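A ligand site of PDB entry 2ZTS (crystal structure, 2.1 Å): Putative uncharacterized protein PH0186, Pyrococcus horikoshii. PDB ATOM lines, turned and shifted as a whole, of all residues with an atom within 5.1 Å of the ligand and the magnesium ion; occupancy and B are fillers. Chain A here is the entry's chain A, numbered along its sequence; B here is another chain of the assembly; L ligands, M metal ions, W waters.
The backbone NH (N) of Thr 41 lies within hydrogen-bond range of an oxygen (O1) of the ligand, at 3.3 Å.
The backbone NH (N) of Gly 40 lies within hydrogen-bond range of an oxygen (O2) of the ligand (2.8 Å).
An oxygen (O1) of the ligand sits at hydrogen-bond distance from the backbone NH of Lys 43 (3.1 Å).
The side-chain amino group (NZ) of Lys 43 is in salt-bridge range of an oxygen (O1) of the ligand.
O2 of the ligand lies within salt-bridge range of NZ of Lys 222 of chain B (2.9 Å).
The side-chain hydroxyl (OG1) of Thr 45 sits at hydrogen-bond distance from an oxygen (O4) of the ligand (2.9 Å).
The guanidinium group (NH2) of Arg 216 is in hydrogen-bond range of an oxygen (O10) of the ligand (3.0 Å).
The backbone NH (N) of Thr 44 sits at hydrogen-bond distance from an oxygen (O4) of the ligand (3.3 Å).
N2 of the ligand sits at hydrogen-bond distance from N of Thr 226 of chain B, at 3.3 Å.
N of Met 223 of chain B lies within hydrogen-bond range of O9 of the ligand (3.0 Å).
An oxygen (O10) of the ligand is in hydrogen-bond range of a ring nitrogen (NE2) of His 228 of chain B (3.1 Å).
OG of Ser 80 sits at hydrogen-bond distance from N3 of the ligand.
N of Gly 42 is in hydrogen-bond range of O6 of the ligand, 3.1 Å away.
The backbone NH (N) of Glu 225 of chain B sits at hydrogen-bond distance from a nitrogen (N2) of the ligand, 3.4 Å away.
O4 of the ligand is in hydrogen-bond range of N of Thr 45 (2.8 Å).
OE2 of Glu 180 is in hydrogen-bond range of OG1 of Thr 39 (2.6 Å).
The side-chain hydroxyl of Thr 44 lies close to the side-chain carboxylate of Asp 142 (2.6 Å).
OG1 of Thr 226 of chain B lies within hydrogen-bond range of O of Arg 224 of chain B, 2.8 Å away.
O of Gly 38 lies within hydrogen-bond range of NZ of Lys 43 (3.0 Å).
The side-chain carboxylate of Glu 225 of chain B is in salt-bridge range of the guanidinium group of Arg 224 of chain B (2.7 Å).
The side-chain carboxylate (OE1) of Glu 180 is in salt-bridge range of the side-chain amino group (NZ) of Lys 43, at 2.7 Å.
NH2 of Arg 216 lies within hydrogen-bond range of SD of Met 230 of chain B, at 3.6 Å.
The guanidinium group of Arg 227 of chain B lies within hydrogen-bond range of the backbone carbonyl oxygen of Ile 237 (2.9 Å).
Gly 38 touches the ligand.
C of Thr 39 touches O2 of the ligand, 3.8 Å away.
CE1 of Phe 81 touches C8 of the ligand, 3.6 Å away.
CD1 of Ile 237 touches O8 of the ligand, 3.5 Å away.
O of Gly 238 touches N4 of the ligand (3.9 Å).
Arg 227 of chain B touches the ligand.
Within 4 Å of the ligand: Gly 38, Thr 39, Gly 40, Thr 41, Gly 42, Lys 43, Thr 44, Thr 45, Ser 80, Phe 81, Arg 216, Ile 237, Gly 238, Lys 222 of chain B, Met 223 of chain B, Glu 225 of chain B, Thr 226 of chain B, Arg 227 of chain B and His 228 of chain B.
OD1 of Asp 142 touches the magnesium ion, at 3.98 Å.
Two residues have an atom within 4 Å of the magnesium ion: Thr 44 and Asp 142.
The magnesium ion is bound by OG1 of Thr 44, 2.0 Å away.
Water W2 is bound to the magnesium ion, 2.0 Å away.
The magnesium ion is bound by O3 of the ligand, at 2.1 Å.
Water W6 binds the magnesium ion, at 2.1 Å.
Water W1 is bound to the magnesium ion, at 2.1 Å.
Water W3 is bound to the magnesium ion.
The magnesium ion has six donor atoms within binding distance.
Water W1 lies within hydrogen-bond range of NZ of Lys 222 of chain B (2.9 Å) and O2 of the ligand (3.5 Å).
Water W2 bridges O2 of the ligand (2.9 Å) and NZ of Lys 222 of chain B (3.4 Å).
Water W5 lies within hydrogen-bond range of an oxygen (O9) of the ligand, the backbone carbonyl oxygen (O) of Gly 40, the guanidinium group (NH2) of Arg 216, the backbone carbonyl oxygen (O) of Arg 221 of chain B and a ring nitrogen (NE2) of His 228 of chain B.
Water W4 lies within hydrogen-bond range of O of Ile 237, NH2 of Arg 216 and N5 of the ligand.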
ATOM      1  N   GLY A  38      37.478  27.699 -31.916  1.00  0.00           N
ATOM      2  CA  GLY A  38      36.589  26.611 -32.283  1.00  0.00           C
ATOM      3  C   GLY A  38      35.154  26.865 -31.829  1.00  0.00           C
ATOM      4  O   GLY A  38      34.832  27.827 -31.088  1.00  0.00           O
ATOM      5  N   THR A  39      34.300  25.960 -32.236  1.00  0.00           N
ATOM      6  CA  THR A  39      32.907  26.032 -31.906  1.00  0.00           C
ATOM      7  C   THR A  39      32.784  26.108 -30.390  1.00  0.00           C
ATOM      8  O   THR A  39      33.418  25.364 -29.689  1.00  0.00           O
ATOM      9  CB  THR A  39      32.165  24.805 -32.459  1.00  0.00           C
ATOM     10  OG1 THR A  39      32.381  24.707 -33.900  1.00  0.00           O
ATOM     11  CG2 THR A  39      30.639  24.974 -32.268  1.00  0.00           C
ATOM     12  N   GLY A  40      31.973  27.017 -29.881  1.00  0.00           N
ATOM     13  CA  GLY A  40      31.675  27.061 -28.470  1.00  0.00           C
ATOM     14  C   GLY A  40      32.773  27.607 -27.601  1.00  0.00           C
ATOM     15  O   GLY A  40      32.760  27.311 -26.403  1.00  0.00           O
ATOM     16  N   THR A  41      33.765  28.326 -28.163  1.00  0.00           N
ATOM     17  CA  THR A  41      34.900  28.855 -27.361  1.00  0.00           C
ATOM     18  C   THR A  41      34.585  30.228 -26.782  1.00  0.00           C
ATOM     19  O   THR A  41      35.321  30.722 -25.931  1.00  0.00           O
ATOM     20  CB  THR A  41      36.207  28.932 -28.136  1.00  0.00           C
ATOM     21  OG1 THR A  41      36.043  29.564 -29.425  1.00  0.00           O
ATOM     22  CG2 THR A  41      36.757  27.519 -28.464  1.00  0.00           C
ATOM     23  N   GLY A  42      33.470  30.828 -27.183  1.00  0.00           N
ATOM     24  CA  GLY A  42      32.955  32.071 -26.619  1.00  0.00           C
ATOM     25  C   GLY A  42      32.997  33.278 -27.520  1.00  0.00           C
ATOM     26  O   GLY A  42      32.934  34.372 -27.088  1.00  0.00           O
ATOM     27  N   LYS A  43      33.120  33.079 -28.827  1.00  0.00           N
ATOM     28  CA  LYS A  43      33.301  34.141 -29.776  1.00  0.00           C
ATOM     29  C   LYS A  43      32.154  35.090 -29.936  1.00  0.00           C
ATOM     30  O   LYS A  43      32.334  36.307 -30.002  1.00  0.00           O
ATOM     31  CB  LYS A  43      33.604  33.566 -31.151  1.00  0.00           C
ATOM     32  CG  LYS A  43      34.863  32.670 -31.202  1.00  0.00           C
ATOM     33  CD  LYS A  43      35.177  32.246 -32.614  1.00  0.00           C
ATOM     34  CE  LYS A  43      34.070  31.447 -33.315  1.00  0.00           C
ATOM     35  NZ  LYS A  43      33.816  30.099 -32.700  1.00  0.00           N
ATOM     36  N   THR A  44      30.973  34.525 -30.133  1.00  0.00           N
ATOM     37  CA  THR A  44      29.772  35.316 -30.250  1.00  0.00           C
ATOM     38  C   THR A  44      29.526  36.092 -28.965  1.00  0.00           C
ATOM     39  O   THR A  44      29.183  37.251 -29.019  1.00  0.00           O
ATOM     40  CB  THR A  44      28.564  34.403 -30.600  1.00  0.00           C
ATOM     41  OG1 THR A  44      28.744  33.983 -31.946  1.00  0.00           O
ATOM     42  CG2 THR A  44      27.202  35.181 -30.608  1.00  0.00           C
ATOM     43  N   THR A  45      29.747  35.450 -27.844  1.00  0.00           N
ATOM     44  CA  THR A  45      29.613  36.092 -26.522  1.00  0.00           C
ATOM     45  C   THR A  45      30.587  37.246 -26.328  1.00  0.00           C
ATOM     46  O   THR A  45      30.185  38.326 -25.951  1.00  0.00           O
ATOM     47  CB  THR A  45      29.718  35.063 -25.453  1.00  0.00           C
ATOM     48  OG1 THR A  45      28.591  34.197 -25.604  1.00  0.00           O
ATOM     49  CG2 THR A  45      29.495  35.647 -24.046  1.00  0.00           C
ATOM     50  N   PHE A  46      31.849  37.009 -26.670  1.00  0.00           N
ATOM     51  CA  PHE A  46      32.888  38.024 -26.622  1.00  0.00           C
ATOM     52  C   PHE A  46      32.512  39.246 -27.488  1.00  0.00           C
ATOM     53  O   PHE A  46      32.606  40.426 -26.996  1.00  0.00           O
ATOM     54  CB  PHE A  46      34.243  37.385 -26.997  1.00  0.00           C
ATOM     55  CG  PHE A  46      35.414  38.202 -26.687  1.00  0.00           C
ATOM     56  CD1 PHE A  46      36.303  37.793 -25.729  1.00  0.00           C
ATOM     57  CD2 PHE A  46      35.661  39.385 -27.352  1.00  0.00           C
ATOM     58  CE1 PHE A  46      37.406  38.510 -25.445  1.00  0.00           C
ATOM     59  CE2 PHE A  46      36.819  40.120 -27.057  1.00  0.00           C
ATOM     60  CZ  PHE A  46      37.677  39.667 -26.106  1.00  0.00           C
ATOM     61  N   GLU A  68      24.925  34.355 -38.535  1.00  0.00           N
ATOM     62  CA  GLU A  68      24.935  33.056 -37.831  1.00  0.00           C
ATOM     63  C   GLU A  68      23.538  32.743 -37.288  1.00  0.00           C
ATOM     64  O   GLU A  68      23.135  31.590 -37.201  1.00  0.00           O
ATOM     65  CB  GLU A  68      25.924  33.068 -36.666  1.00  0.00           C
ATOM     66  CG  GLU A  68      27.415  33.074 -37.081  1.00  0.00           C
ATOM     67  CD  GLU A  68      28.154  31.718 -37.030  1.00  0.00           C
ATOM     68  OE1 GLU A  68      29.235  31.608 -37.640  1.00  0.00           O
ATOM     69  OE2 GLU A  68      27.687  30.776 -36.369  1.00  0.00           O
ATOM     70  N   SER A  80      20.142  36.067 -21.174  1.00  0.00           N
ATOM     71  CA  SER A  80      20.637  35.094 -20.178  1.00  0.00           C
ATOM     72  C   SER A  80      21.835  35.641 -19.379  1.00  0.00           C
ATOM     73  O   SER A  80      22.105  35.111 -18.322  1.00  0.00           O
ATOM     74  CB  SER A  80      20.855  33.633 -20.744  1.00  0.00           C
ATOM     75  OG  SER A  80      22.061  33.371 -21.522  1.00  0.00           O
ATOM     76  N   PHE A  81      22.499  36.704 -19.878  1.00  0.00           N
ATOM     77  CA  PHE A  81      23.647  37.368 -19.197  1.00  0.00           C
ATOM     78  C   PHE A  81      23.310  38.727 -18.598  1.00  0.00           C
ATOM     79  O   PHE A  81      24.203  39.454 -18.210  1.00  0.00           O
ATOM     80  CB  PHE A  81      24.818  37.668 -20.168  1.00  0.00           C
ATOM     81  CG  PHE A  81      25.425  36.456 -20.792  1.00  0.00           C
ATOM     82  CD1 PHE A  81      25.919  35.447 -20.011  1.00  0.00           C
ATOM     83  CD2 PHE A  81      25.527  36.363 -22.143  1.00  0.00           C
ATOM     84  CE1 PHE A  81      26.489  34.337 -20.601  1.00  0.00           C
ATOM     85  CE2 PHE A  81      26.084  35.255 -22.727  1.00  0.00           C
ATOM     86  CZ  PHE A  81      26.550  34.244 -21.955  1.00  0.00           C
ATOM     87  N   ASP A 142      29.838  38.662 -37.258  1.00  0.00           N
ATOM     88  CA  ASP A 142      29.821  37.334 -36.742  1.00  0.00           C
ATOM     89  C   ASP A 142      28.961  36.539 -37.710  1.00  0.00           C
ATOM     90  O   ASP A 142      27.718  36.632 -37.607  1.00  0.00           O
ATOM     91  CB  ASP A 142      29.205  37.354 -35.343  1.00  0.00           C
ATOM     92  CG  ASP A 142      29.310  36.018 -34.648  1.00  0.00           C
ATOM     93  OD1 ASP A 142      28.443  35.740 -33.772  1.00  0.00           O
ATOM     94  OD2 ASP A 142      30.263  35.190 -34.921  1.00  0.00           O
ATOM     95  N   GLU A 180      36.284  30.776 -37.399  1.00  0.00           N
ATOM     96  CA  GLU A 180      36.196  29.523 -36.658  1.00  0.00           C
ATOM     97  C   GLU A 180      37.024  28.434 -37.370  1.00  0.00           C
ATOM     98  O   GLU A 180      36.633  27.974 -38.425  1.00  0.00           O
ATOM     99  CB  GLU A 180      34.717  29.103 -36.559  1.00  0.00           C
ATOM    100  CG  GLU A 180      34.457  27.809 -35.744  1.00  0.00           C
ATOM    101  CD  GLU A 180      33.011  27.695 -35.253  1.00  0.00           C
ATOM    102  OE1 GLU A 180      32.525  28.647 -34.503  1.00  0.00           O
ATOM    103  OE2 GLU A 180      32.370  26.655 -35.592  1.00  0.00           O
ATOM    104  N   ARG A 216      38.618  27.122 -20.370  1.00  0.00           N
ATOM    105  CA  ARG A 216      38.651  28.147 -21.382  1.00  0.00           C
ATOM    106  C   ARG A 216      39.877  29.050 -21.248  1.00  0.00           C
ATOM    107  O   ARG A 216      40.184  29.480 -20.148  1.00  0.00           O
ATOM    108  CB  ARG A 216      37.410  29.034 -21.296  1.00  0.00           C
ATOM    109  CG  ARG A 216      36.088  28.330 -21.310  1.00  0.00           C
ATOM    110  CD  ARG A 216      35.006  29.347 -21.417  1.00  0.00           C
ATOM    111  NE  ARG A 216      33.655  28.807 -21.467  1.00  0.00           N
ATOM    112  CZ  ARG A 216      33.113  28.283 -22.544  1.00  0.00           C
ATOM    113  NH1 ARG A 216      33.802  28.143 -23.655  1.00  0.00           N
ATOM    114  NH2 ARG A 216      31.879  27.813 -22.485  1.00  0.00           N
ATOM    115  N   ILE A 237      32.806  31.965 -18.741  1.00  0.00           N
ATOM    116  CA  ILE A 237      31.598  32.597 -19.237  1.00  0.00           C
ATOM    117  C   ILE A 237      30.567  32.380 -18.129  1.00  0.00           C
ATOM    118  O   ILE A 237      30.123  31.250 -17.925  1.00  0.00           O
ATOM    119  CB  ILE A 237      31.119  31.925 -20.542  1.00  0.00           C
ATOM    120  CG1 ILE A 237      32.228  31.938 -21.602  1.00  0.00           C
ATOM    121  CG2 ILE A 237      29.864  32.594 -21.040  1.00  0.00           C
ATOM    122  CD1 ILE A 237      31.737  31.733 -23.068  1.00  0.00           C
ATOM    123  N   GLY A 238      30.198  33.420 -17.414  1.00  0.00           N
ATOM    124  CA  GLY A 238      29.316  33.294 -16.264  1.00  0.00           C
ATOM    125  C   GLY A 238      27.969  33.979 -16.463  1.00  0.00           C
ATOM    126  O   GLY A 238      27.616  34.244 -17.627  1.00  0.00           O
ATOM    127  N   PRO A 239      27.232  34.266 -15.360  1.00  0.00           N
ATOM    128  CA  PRO A 239      25.949  35.023 -15.446  1.00  0.00           C
ATOM    129  C   PRO A 239      26.077  36.470 -15.918  1.00  0.00           C
ATOM    130  O   PRO A 239      25.117  37.007 -16.490  1.00  0.00           O
ATOM    131  CB  PRO A 239      25.338  34.930 -14.032  1.00  0.00           C
ATOM    132  CG  PRO A 239      26.487  34.420 -13.078  1.00  0.00           C
ATOM    133  CD  PRO A 239      27.582  33.905 -13.968  1.00  0.00           C
ATOM    134  N   ARG B 221      29.889  20.227 -25.498  1.00  0.00           N
ATOM    135  CA  ARG B 221      30.900  21.116 -26.049  1.00  0.00           C
ATOM    136  C   ARG B 221      30.354  22.543 -26.108  1.00  0.00           C
ATOM    137  O   ARG B 221      31.054  23.481 -25.824  1.00  0.00           O
ATOM    138  CB  ARG B 221      31.297  20.557 -27.432  1.00  0.00           C
ATOM    139  CG  ARG B 221      32.152  21.358 -28.341  1.00  0.00           C
ATOM    140  CD  ARG B 221      33.604  21.657 -27.831  1.00  0.00           C
ATOM    141  NE  ARG B 221      34.580  21.076 -28.726  1.00  0.00           N
ATOM    142  CZ  ARG B 221      35.340  21.749 -29.597  1.00  0.00           C
ATOM    143  NH1 ARG B 221      35.292  23.083 -29.739  1.00  0.00           N
ATOM    144  NH2 ARG B 221      36.182  21.037 -30.358  1.00  0.00           N
ATOM    145  N   LYS B 222      29.057  22.653 -26.396  1.00  0.00           N
ATOM    146  CA  LYS B 222      28.372  23.925 -26.609  1.00  0.00           C
ATOM    147  C   LYS B 222      26.880  23.736 -26.273  1.00  0.00           C
ATOM    148  O   LYS B 222      26.277  22.733 -26.655  1.00  0.00           O
ATOM    149  CB  LYS B 222      28.491  24.362 -28.061  1.00  0.00           C
ATOM    150  CG  LYS B 222      27.898  25.706 -28.357  1.00  0.00           C
ATOM    151  CD  LYS B 222      28.100  26.138 -29.817  1.00  0.00           C
ATOM    152  CE  LYS B 222      27.224  27.336 -30.081  1.00  0.00           C
ATOM    153  NZ  LYS B 222      27.712  28.277 -31.061  1.00  0.00           N
ATOM    154  N   MET B 223      26.308  24.661 -25.534  1.00  0.00           N
ATOM    155  CA  MET B 223      24.831  24.672 -25.406  1.00  0.00           C
ATOM    156  C   MET B 223      24.389  26.083 -25.132  1.00  0.00           C
ATOM    157  O   MET B 223      24.752  26.631 -24.098  1.00  0.00           O
ATOM    158  CB  MET B 223      24.365  23.762 -24.292  1.00  0.00           C
ATOM    159  CG  MET B 223      22.826  23.615 -24.152  1.00  0.00           C
ATOM    160  SD  MET B 223      22.068  22.746 -25.770  1.00  0.00           S
ATOM    161  CE  MET B 223      23.137  21.049 -25.669  1.00  0.00           C
ATOM    162  N   ARG B 224      23.620  26.670 -26.023  1.00  0.00           N
ATOM    163  CA  ARG B 224      23.244  28.060 -25.866  1.00  0.00           C
ATOM    164  C   ARG B 224      22.392  28.237 -24.598  1.00  0.00           C
ATOM    165  O   ARG B 224      21.753  27.307 -24.135  1.00  0.00           O
ATOM    166  CB  ARG B 224      22.508  28.563 -27.103  1.00  0.00           C
ATOM    167  CG  ARG B 224      21.053  28.016 -27.264  1.00  0.00           C
ATOM    168  CD  ARG B 224      20.076  29.044 -27.886  1.00  0.00           C
ATOM    169  NE  ARG B 224      18.751  28.449 -28.065  1.00  0.00           N
ATOM    170  CZ  ARG B 224      17.782  28.890 -28.874  1.00  0.00           C
ATOM    171  NH1 ARG B 224      17.915  30.005 -29.580  1.00  0.00           N
ATOM    172  NH2 ARG B 224      16.652  28.197 -28.933  1.00  0.00           N
ATOM    173  N   GLU B 225      22.461  29.438 -24.032  1.00  0.00           N
ATOM    174  CA  GLU B 225      21.653  29.829 -22.868  1.00  0.00           C
ATOM    175  C   GLU B 225      21.861  28.923 -21.681  1.00  0.00           C
ATOM    176  O   GLU B 225      20.972  28.791 -20.872  1.00  0.00           O
ATOM    177  CB  GLU B 225      20.131  29.870 -23.212  1.00  0.00           C
ATOM    178  CG  GLU B 225      19.742  30.798 -24.351  1.00  0.00           C
ATOM    179  CD  GLU B 225      18.291  30.624 -24.864  1.00  0.00           C
ATOM    180  OE1 GLU B 225      18.089  29.902 -25.895  1.00  0.00           O
ATOM    181  OE2 GLU B 225      17.333  31.226 -24.281  1.00  0.00           O
ATOM    182  N   THR B 226      23.000  28.266 -21.568  1.00  0.00           N
ATOM    183  CA  THR B 226      23.155  27.303 -20.507  1.00  0.00           C
ATOM    184  C   THR B 226      24.568  27.293 -19.977  1.00  0.00           C
ATOM    185  O   THR B 226      25.497  27.171 -20.744  1.00  0.00           O
ATOM    186  CB  THR B 226      22.841  25.888 -21.065  1.00  0.00           C
ATOM    187  OG1 THR B 226      21.613  25.891 -21.779  1.00  0.00           O
ATOM    188  CG2 THR B 226      22.599  24.904 -19.953  1.00  0.00           C
ATOM    189  N   ARG B 227      24.709  27.323 -18.669  1.00  0.00           N
ATOM    190  CA  ARG B 227      25.973  27.069 -17.968  1.00  0.00           C
ATOM    191  C   ARG B 227      26.007  25.553 -17.854  1.00  0.00           C
ATOM    192  O   ARG B 227      25.512  25.017 -16.860  1.00  0.00           O
ATOM    193  CB  ARG B 227      25.988  27.796 -16.571  1.00  0.00           C
ATOM    194  CG  ARG B 227      27.335  27.843 -15.709  1.00  0.00           C
ATOM    195  CD  ARG B 227      27.455  29.158 -14.797  1.00  0.00           C
ATOM    196  NE  ARG B 227      28.664  29.421 -13.961  1.00  0.00           N
ATOM    197  CZ  ARG B 227      29.941  29.597 -14.389  1.00  0.00           C
ATOM    198  NH1 ARG B 227      30.281  29.501 -15.662  1.00  0.00           N
ATOM    199  NH2 ARG B 227      30.909  29.872 -13.513  1.00  0.00           N
ATOM    200  N   HIS B 228      26.516  24.878 -18.888  1.00  0.00           N
ATOM    201  CA  HIS B 228      26.611  23.385 -18.923  1.00  0.00           C
ATOM    202  C   HIS B 228      27.951  22.942 -18.386  1.00  0.00           C
ATOM    203  O   HIS B 228      28.924  23.629 -18.526  1.00  0.00           O
ATOM    204  CB  HIS B 228      26.439  22.769 -20.352  1.00  0.00           C
ATOM    205  CG  HIS B 228      27.384  23.330 -21.388  1.00  0.00           C
ATOM    206  ND1 HIS B 228      28.710  23.550 -21.144  1.00  0.00           N
ATOM    207  CD2 HIS B 228      27.192  23.697 -22.673  1.00  0.00           C
ATOM    208  CE1 HIS B 228      29.291  24.070 -22.218  1.00  0.00           C
ATOM    209  NE2 HIS B 228      28.387  24.172 -23.156  1.00  0.00           N
ATOM    210  N   MET B 230      31.453  21.131 -18.470  1.00  0.00           N
ATOM    211  CA  MET B 230      32.445  21.033 -19.524  1.00  0.00           C
ATOM    212  C   MET B 230      33.303  19.766 -19.395  1.00  0.00           C
ATOM    213  O   MET B 230      34.250  19.625 -20.153  1.00  0.00           O
ATOM    214  CB  MET B 230      33.415  22.235 -19.441  1.00  0.00           C
ATOM    215  CG  MET B 230      32.804  23.636 -19.372  1.00  0.00           C
ATOM    216  SD  MET B 230      32.658  24.522 -21.187  1.00  0.00           S
ATOM    217  CE  MET B 230      33.636  23.365 -22.547  1.00  0.00           C
HETATM  218  P1  LIG L   1      31.021  30.417 -30.190  1.00  0.00           P
HETATM  219  O1  LIG L   1      32.517  30.457 -30.382  1.00  0.00           O
HETATM  220  O2  LIG L   1      30.452  29.131 -30.785  1.00  0.00           O
HETATM  221  O3  LIG L   1      30.452  31.558 -30.982  1.00  0.00           O
HETATM  222  P2  LIG L   1      29.463  31.201 -27.935  1.00  0.00           P
HETATM  223  O4  LIG L   1      29.889  32.622 -27.692  1.00  0.00           O
HETATM  224  O5  LIG L   1      28.318  30.968 -28.885  1.00  0.00           O
HETATM  225  O6  LIG L   1      30.716  30.362 -28.619  1.00  0.00           O
HETATM  226  O7  LIG L   1      29.414  30.570 -26.486  1.00  0.00           O
HETATM  227  C1  LIG L   1      28.284  29.880 -26.043  1.00  0.00           C
HETATM  228  C2  LIG L   1      28.688  29.176 -24.786  1.00  0.00           C
HETATM  229  O8  LIG L   1      28.688  30.049 -23.676  1.00  0.00           O
HETATM  230  C3  LIG L   1      27.761  28.011 -24.493  1.00  0.00           C
HETATM  231  O9  LIG L   1      28.273  26.901 -25.148  1.00  0.00           O
HETATM  232  C4  LIG L   1      27.872  27.929 -23.006  1.00  0.00           C
HETATM  233  O10 LIG L   1      28.928  27.139 -22.579  1.00  0.00           O
HETATM  234  C5  LIG L   1      28.158  29.355 -22.568  1.00  0.00           C
HETATM  235  N1  LIG L   1      26.903  29.985 -22.153  1.00  0.00           N
HETATM  236  C6  LIG L   1      25.866  30.374 -22.976  1.00  0.00           C
HETATM  237  N2  LIG L   1      24.902  30.936 -22.195  1.00  0.00           N
HETATM  238  C7  LIG L   1      25.326  30.879 -20.910  1.00  0.00           C
HETATM  239  C8  LIG L   1      24.711  31.310 -19.750  1.00  0.00           C
HETATM  240  N3  LIG L   1      23.670  32.133 -19.868  1.00  0.00           N
HETATM  241  N4  LIG L   1      25.411  31.159 -18.578  1.00  0.00           N
HETATM  242  C9  LIG L   1      26.689  30.561 -18.563  1.00  0.00           C
HETATM  243  N5  LIG L   1      27.293  30.120 -19.743  1.00  0.00           N
HETATM  244  C10 LIG L   1      26.597  30.293 -20.878  1.00  0.00           C
HETATM  245 MG    MG M   1      29.032  32.053 -32.390  1.00  0.00          MG
HETATM  246  O   HOH W   1      27.651  31.174 -31.097  1.00  0.00           O
HETATM  247  O   HOH W   2      29.383  30.263 -33.252  1.00  0.00           O
HETATM  248  O   HOH W   3      27.489  32.225 -33.786  1.00  0.00           O
HETATM  249  O   HOH W   4      30.233  28.477 -19.648  1.00  0.00           O
HETATM  250  O   HOH W   5      30.581  26.318 -24.797  1.00  0.00           O
HETATM  251  O   HOH W   6      30.421  32.791 -33.757  1.00  0.00           O
